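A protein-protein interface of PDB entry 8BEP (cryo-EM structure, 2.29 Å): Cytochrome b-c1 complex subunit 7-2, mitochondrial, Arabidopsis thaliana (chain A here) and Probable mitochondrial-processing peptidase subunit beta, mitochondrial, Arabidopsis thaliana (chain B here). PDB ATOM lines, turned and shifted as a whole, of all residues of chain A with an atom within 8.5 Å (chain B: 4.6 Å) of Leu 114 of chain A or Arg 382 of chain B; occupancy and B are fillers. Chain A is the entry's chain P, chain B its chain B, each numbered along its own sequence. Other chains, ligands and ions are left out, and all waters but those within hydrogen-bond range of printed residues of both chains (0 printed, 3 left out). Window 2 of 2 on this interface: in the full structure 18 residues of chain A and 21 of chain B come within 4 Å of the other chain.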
ATOM      1  N   GLU A 104     -17.385   6.323 -15.171  1.00  0.00           N
ATOM      2  CA  GLU A 104     -18.247   7.217 -15.941  1.00  0.00           C
ATOM      3  C   GLU A 104     -18.334   8.595 -15.291  1.00  0.00           C
ATOM      4  O   GLU A 104     -18.322   9.621 -15.983  1.00  0.00           O
ATOM      5  CB  GLU A 104     -19.636   6.601 -16.099  1.00  0.00           C
ATOM      6  CG  GLU A 104     -19.724   5.603 -17.237  1.00  0.00           C
ATOM      7  CD  GLU A 104     -21.047   4.867 -17.278  1.00  0.00           C
ATOM      8  OE1 GLU A 104     -22.010   5.334 -16.637  1.00  0.00           O
ATOM      9  OE2 GLU A 104     -21.125   3.823 -17.960  1.00  0.00           O
ATOM     10  N   ARG A 105     -18.392   8.609 -13.955  1.00  0.00           N
ATOM     11  CA  ARG A 105     -18.432   9.886 -13.195  1.00  0.00           C
ATOM     12  C   ARG A 105     -17.160  10.682 -13.484  1.00  0.00           C
ATOM     13  O   ARG A 105     -17.272  11.890 -13.766  1.00  0.00           O
ATOM     14  CB  ARG A 105     -18.522   9.574 -11.699  1.00  0.00           C
ATOM     15  CG  ARG A 105     -18.696  10.791 -10.802  1.00  0.00           C
ATOM     16  CD  ARG A 105     -20.145  11.225 -10.791  1.00  0.00           C
ATOM     17  NE  ARG A 105     -20.417  12.286  -9.835  1.00  0.00           N
ATOM     18  CZ  ARG A 105     -21.614  12.824  -9.633  1.00  0.00           C
ATOM     19  NH1 ARG A 105     -22.659  12.395 -10.319  1.00  0.00           N
ATOM     20  NH2 ARG A 105     -21.762  13.779  -8.732  1.00  0.00           N
ATOM     21  N   GLU A 107     -15.107  10.435 -16.040  1.00  0.00           N
ATOM     22  CA  GLU A 107     -15.097  10.884 -17.429  1.00  0.00           C
ATOM     23  C   GLU A 107     -15.974  12.117 -17.612  1.00  0.00           C
ATOM     24  O   GLU A 107     -15.597  13.056 -18.323  1.00  0.00           O
ATOM     25  CB  GLU A 107     -15.547   9.748 -18.349  1.00  0.00           C
ATOM     26  CG  GLU A 107     -15.816  10.166 -19.786  1.00  0.00           C
ATOM     27  CD  GLU A 107     -16.506   9.079 -20.593  1.00  0.00           C
ATOM     28  OE1 GLU A 107     -17.635   8.691 -20.231  1.00  0.00           O
ATOM     29  OE2 GLU A 107     -15.922   8.616 -21.591  1.00  0.00           O
ATOM     30  N   ARG A 108     -17.143  12.138 -16.968  1.00  0.00           N
ATOM     31  CA  ARG A 108     -17.984  13.331 -17.008  1.00  0.00           C
ATOM     32  C   ARG A 108     -17.269  14.536 -16.406  1.00  0.00           C
ATOM     33  O   ARG A 108     -17.331  15.642 -16.953  1.00  0.00           O
ATOM     34  CB  ARG A 108     -19.298  13.076 -16.272  1.00  0.00           C
ATOM     35  CG  ARG A 108     -20.337  12.341 -17.074  1.00  0.00           C
ATOM     36  CD  ARG A 108     -21.679  12.402 -16.377  1.00  0.00           C
ATOM     37  NE  ARG A 108     -22.434  13.586 -16.766  1.00  0.00           N
ATOM     38  CZ  ARG A 108     -23.120  13.695 -17.894  1.00  0.00           C
ATOM     39  NH1 ARG A 108     -23.159  12.712 -18.775  1.00  0.00           N
ATOM     40  NH2 ARG A 108     -23.786  14.816 -18.142  1.00  0.00           N
ATOM     41  N   GLU A 109     -16.593  14.342 -15.273  1.00  0.00           N
ATOM     42  CA  GLU A 109     -15.901  15.457 -14.629  1.00  0.00           C
ATOM     43  C   GLU A 109     -14.759  15.984 -15.493  1.00  0.00           C
ATOM     44  O   GLU A 109     -14.537  17.199 -15.560  1.00  0.00           O
ATOM     45  CB  GLU A 109     -15.383  15.039 -13.255  1.00  0.00           C
ATOM     46  CG  GLU A 109     -16.436  15.029 -12.167  1.00  0.00           C
ATOM     47  CD  GLU A 109     -16.634  16.390 -11.528  1.00  0.00           C
ATOM     48  OE1 GLU A 109     -15.896  17.332 -11.884  1.00  0.00           O
ATOM     49  OE2 GLU A 109     -17.529  16.516 -10.666  1.00  0.00           O
ATOM     50  N   LEU A 111     -14.421  16.146 -18.727  1.00  0.00           N
ATOM     51  CA  LEU A 111     -14.851  16.878 -19.909  1.00  0.00           C
ATOM     52  C   LEU A 111     -15.701  18.097 -19.578  1.00  0.00           C
ATOM     53  O   LEU A 111     -16.208  18.749 -20.493  1.00  0.00           O
ATOM     54  CB  LEU A 111     -15.607  15.946 -20.853  1.00  0.00           C
ATOM     55  CG  LEU A 111     -14.680  15.016 -21.637  1.00  0.00           C
ATOM     56  CD1 LEU A 111     -15.473  14.064 -22.512  1.00  0.00           C
ATOM     57  CD2 LEU A 111     -13.710  15.833 -22.467  1.00  0.00           C
ATOM     58  N   GLY A 112     -15.863  18.418 -18.298  1.00  0.00           N
ATOM     59  CA  GLY A 112     -16.585  19.610 -17.906  1.00  0.00           C
ATOM     60  C   GLY A 112     -18.090  19.506 -17.938  1.00  0.00           C
ATOM     61  O   GLY A 112     -18.763  20.534 -18.048  1.00  0.00           O
ATOM     62  N   ALA A 113     -18.645  18.302 -17.846  1.00  0.00           N
ATOM     63  CA  ALA A 113     -20.085  18.110 -17.846  1.00  0.00           C
ATOM     64  C   ALA A 113     -20.642  18.138 -16.428  1.00  0.00           C
ATOM     65  O   ALA A 113     -19.936  17.893 -15.447  1.00  0.00           O
ATOM     66  CB  ALA A 113     -20.459  16.790 -18.522  1.00  0.00           C
ATOM     67  N   LEU A 114     -21.933  18.445 -16.335  1.00  0.00           N
ATOM     68  CA  LEU A 114     -22.623  18.434 -15.056  1.00  0.00           C
ATOM     69  C   LEU A 114     -22.767  17.004 -14.535  1.00  0.00           C
ATOM     70  O   LEU A 114     -22.866  16.058 -15.318  1.00  0.00           O
ATOM     71  CB  LEU A 114     -24.004  19.072 -15.190  1.00  0.00           C
ATOM     72  CG  LEU A 114     -24.036  20.561 -15.526  1.00  0.00           C
ATOM     73  CD1 LEU A 114     -25.467  21.035 -15.729  1.00  0.00           C
ATOM     74  CD2 LEU A 114     -23.346  21.371 -14.446  1.00  0.00           C
ATOM     75  N   PRO A 115     -22.775  16.822 -13.215  1.00  0.00           N
ATOM     76  CA  PRO A 115     -23.002  15.483 -12.659  1.00  0.00           C
ATOM     77  C   PRO A 115     -24.399  14.980 -12.985  1.00  0.00           C
ATOM     78  O   PRO A 115     -25.353  15.752 -13.087  1.00  0.00           O
ATOM     79  CB  PRO A 115     -22.825  15.684 -11.148  1.00  0.00           C
ATOM     80  CG  PRO A 115     -22.164  17.003 -10.992  1.00  0.00           C
ATOM     81  CD  PRO A 115     -22.557  17.829 -12.165  1.00  0.00           C
ATOM     82  N   LEU A 116     -24.512  13.663 -13.150  1.00  0.00           N
ATOM     83  CA  LEU A 116     -25.802  13.043 -13.420  1.00  0.00           C
ATOM     84  C   LEU A 116     -26.674  12.935 -12.178  1.00  0.00           C
ATOM     85  O   LEU A 116     -27.867  12.642 -12.305  1.00  0.00           O
ATOM     86  CB  LEU A 116     -25.604  11.653 -14.027  1.00  0.00           C
ATOM     87  CG  LEU A 116     -25.135  11.582 -15.479  1.00  0.00           C
ATOM     88  CD1 LEU A 116     -24.971  10.134 -15.910  1.00  0.00           C
ATOM     89  CD2 LEU A 116     -26.086  12.323 -16.411  1.00  0.00           C
ATOM     90  N   TYR A 117     -26.108  13.153 -10.995  1.00  0.00           N
ATOM     91  CA  TYR A 117     -26.845  13.106  -9.742  1.00  0.00           C
ATOM     92  C   TYR A 117     -25.982  13.746  -8.667  1.00  0.00           C
ATOM     93  O   TYR A 117     -24.752  13.745  -8.757  1.00  0.00           O
ATOM     94  CB  TYR A 117     -27.224  11.668  -9.365  1.00  0.00           C
ATOM     95  CG  TYR A 117     -26.099  10.684  -9.572  1.00  0.00           C
ATOM     96  CD1 TYR A 117     -25.097  10.538  -8.626  1.00  0.00           C
ATOM     97  CD2 TYR A 117     -26.030   9.914 -10.723  1.00  0.00           C
ATOM     98  CE1 TYR A 117     -24.063   9.647  -8.813  1.00  0.00           C
ATOM     99  CE2 TYR A 117     -24.999   9.020 -10.921  1.00  0.00           C
ATOM    100  CZ  TYR A 117     -24.017   8.892  -9.962  1.00  0.00           C
ATOM    101  OH  TYR A 117     -22.991   8.004 -10.153  1.00  0.00           O
ATOM    102  N   GLN A 118     -26.605  14.239  -7.636  1.00  0.00           N
ATOM    103  CA  GLN A 118     -25.881  14.954  -6.590  1.00  0.00           C
ATOM    104  C   GLN A 118     -26.593  14.618  -5.299  1.00  0.00           C
ATOM    105  O   GLN A 118     -27.779  14.324  -5.336  1.00  0.00           O
ATOM    106  CB  GLN A 118     -25.688  16.473  -6.751  1.00  0.00           C
ATOM    107  CG  GLN A 118     -25.097  17.007  -8.028  1.00  0.00           C
ATOM    108  CD  GLN A 118     -25.380  18.487  -8.073  1.00  0.00           C
ATOM    109  OE1 GLN A 118     -26.513  18.911  -8.257  1.00  0.00           O
ATOM    110  NE2 GLN A 118     -24.355  19.292  -7.897  1.00  0.00           N
ATOM    111  N   ASP B 378     -24.992  23.393 -20.702  1.00  0.00           N
ATOM    112  CA  ASP B 378     -25.371  23.081 -19.329  1.00  0.00           C
ATOM    113  C   ASP B 378     -26.874  23.211 -19.107  1.00  0.00           C
ATOM    114  O   ASP B 378     -27.447  22.449 -18.324  1.00  0.00           O
ATOM    115  CB  ASP B 378     -24.614  23.983 -18.359  1.00  0.00           C
ATOM    116  CG  ASP B 378     -23.202  23.509 -18.104  1.00  0.00           C
ATOM    117  OD1 ASP B 378     -22.987  22.284 -18.037  1.00  0.00           O
ATOM    118  OD2 ASP B 378     -22.305  24.363 -17.962  1.00  0.00           O
ATOM    119  N   LEU B 379     -27.525  24.171 -19.768  1.00  0.00           N
ATOM    120  CA  LEU B 379     -28.971  24.314 -19.629  1.00  0.00           C
ATOM    121  C   LEU B 379     -29.699  23.078 -20.149  1.00  0.00           C
ATOM    122  O   LEU B 379     -30.594  22.538 -19.485  1.00  0.00           O
ATOM    123  CB  LEU B 379     -29.440  25.572 -20.362  1.00  0.00           C
ATOM    124  CG  LEU B 379     -30.949  25.794 -20.463  1.00  0.00           C
ATOM    125  CD1 LEU B 379     -31.546  25.977 -19.081  1.00  0.00           C
ATOM    126  CD2 LEU B 379     -31.248  26.992 -21.343  1.00  0.00           C
ATOM    127  N   THR B 380     -29.314  22.610 -21.339  1.00  0.00           N
ATOM    128  CA  THR B 380     -29.896  21.386 -21.875  1.00  0.00           C
ATOM    129  C   THR B 380     -29.598  20.198 -20.971  1.00  0.00           C
ATOM    130  O   THR B 380     -30.456  19.334 -20.772  1.00  0.00           O
ATOM    131  CB  THR B 380     -29.379  21.124 -23.288  1.00  0.00           C
ATOM    132  OG1 THR B 380     -29.713  22.227 -24.136  1.00  0.00           O
ATOM    133  CG2 THR B 380     -29.996  19.855 -23.858  1.00  0.00           C
ATOM    134  N   GLN B 381     -28.388  20.144 -20.409  1.00  0.00           N
ATOM    135  CA  GLN B 381     -28.051  19.061 -19.492  1.00  0.00           C
ATOM    136  C   GLN B 381     -28.975  19.065 -18.282  1.00  0.00           C
ATOM    137  O   GLN B 381     -29.511  18.026 -17.900  1.00  0.00           O
ATOM    138  CB  GLN B 381     -26.595  19.178 -19.049  1.00  0.00           C
ATOM    139  CG  GLN B 381     -25.601  18.530 -19.980  1.00  0.00           C
ATOM    140  CD  GLN B 381     -24.176  18.713 -19.501  1.00  0.00           C
ATOM    141  OE1 GLN B 381     -23.645  17.879 -18.773  1.00  0.00           O
ATOM    142  NE2 GLN B 381     -23.555  19.813 -19.902  1.00  0.00           N
ATOM    143  N   ARG B 382     -29.181  20.233 -17.673  1.00  0.00           N
ATOM    144  CA  ARG B 382     -30.043  20.315 -16.498  1.00  0.00           C
ATOM    145  C   ARG B 382     -31.465  19.883 -16.838  1.00  0.00           C
ATOM    146  O   ARG B 382     -32.071  19.066 -16.128  1.00  0.00           O
ATOM    147  CB  ARG B 382     -30.020  21.740 -15.944  1.00  0.00           C
ATOM    148  CG  ARG B 382     -28.917  21.992 -14.934  1.00  0.00           C
ATOM    149  CD  ARG B 382     -28.760  23.468 -14.620  1.00  0.00           C
ATOM    150  NE  ARG B 382     -27.391  23.821 -14.264  1.00  0.00           N
ATOM    151  CZ  ARG B 382     -26.798  23.488 -13.123  1.00  0.00           C
ATOM    152  NH1 ARG B 382     -27.426  22.787 -12.195  1.00  0.00           N
ATOM    153  NH2 ARG B 382     -25.542  23.868 -12.910  1.00  0.00           N
ATOM    154  N   VAL B 383     -31.987  20.384 -17.959  1.00  0.00           N
ATOM    155  CA  VAL B 383     -33.365  20.086 -18.343  1.00  0.00           C
ATOM    156  C   VAL B 383     -33.535  18.598 -18.628  1.00  0.00           C
ATOM    157  O   VAL B 383     -34.492  17.969 -18.167  1.00  0.00           O
ATOM    158  CB  VAL B 383     -33.782  20.952 -19.546  1.00  0.00           C
ATOM    159  CG1 VAL B 383     -35.069  20.434 -20.159  1.00  0.00           C
ATOM    160  CG2 VAL B 383     -33.927  22.402 -19.118  1.00  0.00           C
ATOM    161  N   ALA B 384     -32.604  18.009 -19.383  1.00  0.00           N
ATOM    162  CA  ALA B 384     -32.734  16.604 -19.754  1.00  0.00           C
ATOM    163  C   ALA B 384     -32.455  15.673 -18.581  1.00  0.00           C
ATOM    164  O   ALA B 384     -33.079  14.614 -18.474  1.00  0.00           O
ATOM    165  CB  ALA B 384     -31.804  16.276 -20.922  1.00  0.00           C
ATOM    166  N   ILE B 385     -31.524  16.040 -17.700  1.00  0.00           N
ATOM    167  CA  ILE B 385     -31.172  15.180 -16.578  1.00  0.00           C
ATOM    168  C   ILE B 385     -32.292  15.155 -15.548  1.00  0.00           C
ATOM    169  O   ILE B 385     -32.550  14.120 -14.923  1.00  0.00           O
ATOM    170  CB  ILE B 385     -29.830  15.629 -15.968  1.00  0.00           C
ATOM    171  CG1 ILE B 385     -28.668  15.117 -16.821  1.00  0.00           C
ATOM    172  CG2 ILE B 385     -29.681  15.136 -14.536  1.00  0.00           C
ATOM    173  CD1 ILE B 385     -27.408  15.934 -16.702  1.00  0.00           C
ATOM    174  N   ASN B 386     -32.982  16.278 -15.348  1.00  0.00           N
ATOM    175  CA  ASN B 386     -34.023  16.300 -14.330  1.00  0.00           C
ATOM    176  C   ASN B 386     -35.444  16.208 -14.884  1.00  0.00           C
ATOM    177  O   ASN B 386     -36.393  16.234 -14.097  1.00  0.00           O
ATOM    178  CB  ASN B 386     -33.867  17.544 -13.457  1.00  0.00           C
ATOM    179  CG  ASN B 386     -32.496  17.620 -12.809  1.00  0.00           C
ATOM    180  OD1 ASN B 386     -32.302  17.145 -11.696  1.00  0.00           O
ATOM    181  ND2 ASN B 386     -31.542  18.221 -13.504  1.00  0.00           N
ATOM    182  N   ILE B 388     -37.468  18.308 -16.713  1.00  0.00           N
ATOM    183  CA  ILE B 388     -38.203  19.462 -16.215  1.00  0.00           C
ATOM    184  C   ILE B 388     -38.784  20.306 -17.350  1.00  0.00           C
ATOM    185  O   ILE B 388     -39.153  21.451 -17.135  1.00  0.00           O
ATOM    186  CB  ILE B 388     -37.328  20.313 -15.276  1.00  0.00           C
ATOM    187  CG1 ILE B 388     -36.036  20.732 -15.977  1.00  0.00           C
ATOM    188  CG2 ILE B 388     -37.032  19.554 -13.994  1.00  0.00           C
ATOM    189  CD1 ILE B 388     -35.207  21.709 -15.185  1.00  0.00           C
ATOM    190  N   ALA B 422     -33.483  27.120 -13.516  1.00  0.00           N
ATOM    191  CA  ALA B 422     -32.395  26.623 -14.356  1.00  0.00           C
ATOM    192  C   ALA B 422     -32.106  27.567 -15.518  1.00  0.00           C
ATOM    193  O   ALA B 422     -30.940  27.857 -15.817  1.00  0.00           O
ATOM    194  CB  ALA B 422     -32.724  25.225 -14.877  1.00  0.00           C
ATOM    195  N   TYR B 425     -30.431  30.719 -14.178  1.00  0.00           N
ATOM    196  CA  TYR B 425     -29.083  30.403 -13.725  1.00  0.00           C
ATOM    197  C   TYR B 425     -28.123  30.286 -14.898  1.00  0.00           C
ATOM    198  O   TYR B 425     -27.056  30.907 -14.903  1.00  0.00           O
ATOM    199  CB  TYR B 425     -29.087  29.108 -12.910  1.00  0.00           C
ATOM    200  CG  TYR B 425     -27.747  28.776 -12.288  1.00  0.00           C
ATOM    201  CD1 TYR B 425     -27.386  29.294 -11.053  1.00  0.00           C
ATOM    202  CD2 TYR B 425     -26.840  27.949 -12.941  1.00  0.00           C
ATOM    203  CE1 TYR B 425     -26.162  28.995 -10.482  1.00  0.00           C
ATOM    204  CE2 TYR B 425     -25.613  27.650 -12.381  1.00  0.00           C
ATOM    205  CZ  TYR B 425     -25.281  28.173 -11.151  1.00  0.00           C
ATOM    206  OH  TYR B 425     -24.064  27.877 -10.591  1.00  0.00           O
ATOM    207  N   GLU B 426     -28.500  29.515 -15.920  1.00  0.00           N
ATOM    208  CA  GLU B 426     -27.571  29.280 -17.018  1.00  0.00           C
ATOM    209  C   GLU B 426     -27.414  30.508 -17.906  1.00  0.00           C
ATOM    210  O   GLU B 426     -26.348  30.702 -18.498  1.00  0.00           O
ATOM    211  CB  GLU B 426     -28.003  28.064 -17.838  1.00  0.00           C
ATOM    212  CG  GLU B 426     -27.852  26.731 -17.105  1.00  0.00           C
ATOM    213  CD  GLU B 426     -26.410  26.393 -16.724  1.00  0.00           C
ATOM    214  OE1 GLU B 426     -25.470  27.036 -17.232  1.00  0.00           O
ATOM    215  OE2 GLU B 426     -26.219  25.468 -15.911  1.00  0.00           O
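CB of Ala 113 of chain A touches OE1 of Gln 381 of chain B, at 3.4 Å. Asp 378 of chain B touches Leu 114 of chain A (OD1 to CG, 3.2 Å). Arg 382 of chain B touches Leu 114 of chain A (NH2 to CD2, 3.7 Å). Leu 116 of chain A touches Ile 385 of chain B (O to CG2, 3.8 Å).
Of chain B, only Asp 378, Gln 381 and Arg 382 come within 4 Å of Leu 114 of chain A. Of chain A, only Leu 114 comes within 4 Å of Arg 382 of chain B. Printed residues of chain A within 4 Å of Ile 385 of chain B: Leu 116 (3.8 Å). Of the printed residues of chain A, Gln 381 of chain B touches Arg 108 (3.1 Å), Ala 113 (3.4 Å) and Leu 114 (3.0 Å). Of the printed residues of chain B, Arg 108 of chain A touches Gln 381 (3.1 Å). Of the printed residues of chain A, Asp 378 of chain B touches Leu 114. The nearest residue of chain B that does not touch Leu 114 of chain A is Glu 426 of chain B (4.5 Å).
The backbone carbonyl oxygen (O) of Arg 108 of chain A sits at hydrogen-bond distance from the backbone NH (N) of Ala 113 of chain A. The guanidinium group of Arg 108 of chain A is in hydrogen-bond range of the backbone carbonyl oxygen of Leu 114 of chain A (2.9 Å). The backbone carbonyl oxygen (O) of Arg 382 of chain B is in hydrogen-bond range of the side-chain amide nitrogen (ND2) of Asn 386 of chain B (2.8 Å). The side-chain amide nitrogen of Gln 381 of chain B is in hydrogen-bond range of the side-chain carboxylate of Asp 378 of chain B (3.1 Å). The side-chain carboxylate of Glu 426 of chain B is in salt-bridge range of the guanidinium group of Arg 382 of chain B (2.6 Å).
Printed residues of chain B that touch a printed residue of chain A: Asp 378, Gln 381, Arg 382 and Ile 385. Hydrophobic or aromatic side chains of chain B that line the printed part of chain A: Ile 385. Printed residues of chain A that touch a printed residue of chain B: Arg 108, Ala 113, Leu 114 and Leu 116. Hydrophobic or aromatic side chains of chain A that line the printed part of chain B: Ala 113, Leu 114 and Leu 116. Among the printed residues, no Asp or Glu carboxylate lies within 4 Å of a Lys or Arg side-chain nitrogen of the other chain.
OE1 of Gln 381 of chain B lies within hydrogen-bond range of NH2 of Arg 108 of chain A (3.1 Å). N of Leu 114 of chain A is in hydrogen-bond range of OE1 of Gln 381 of chain B, 3.0 Å away.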
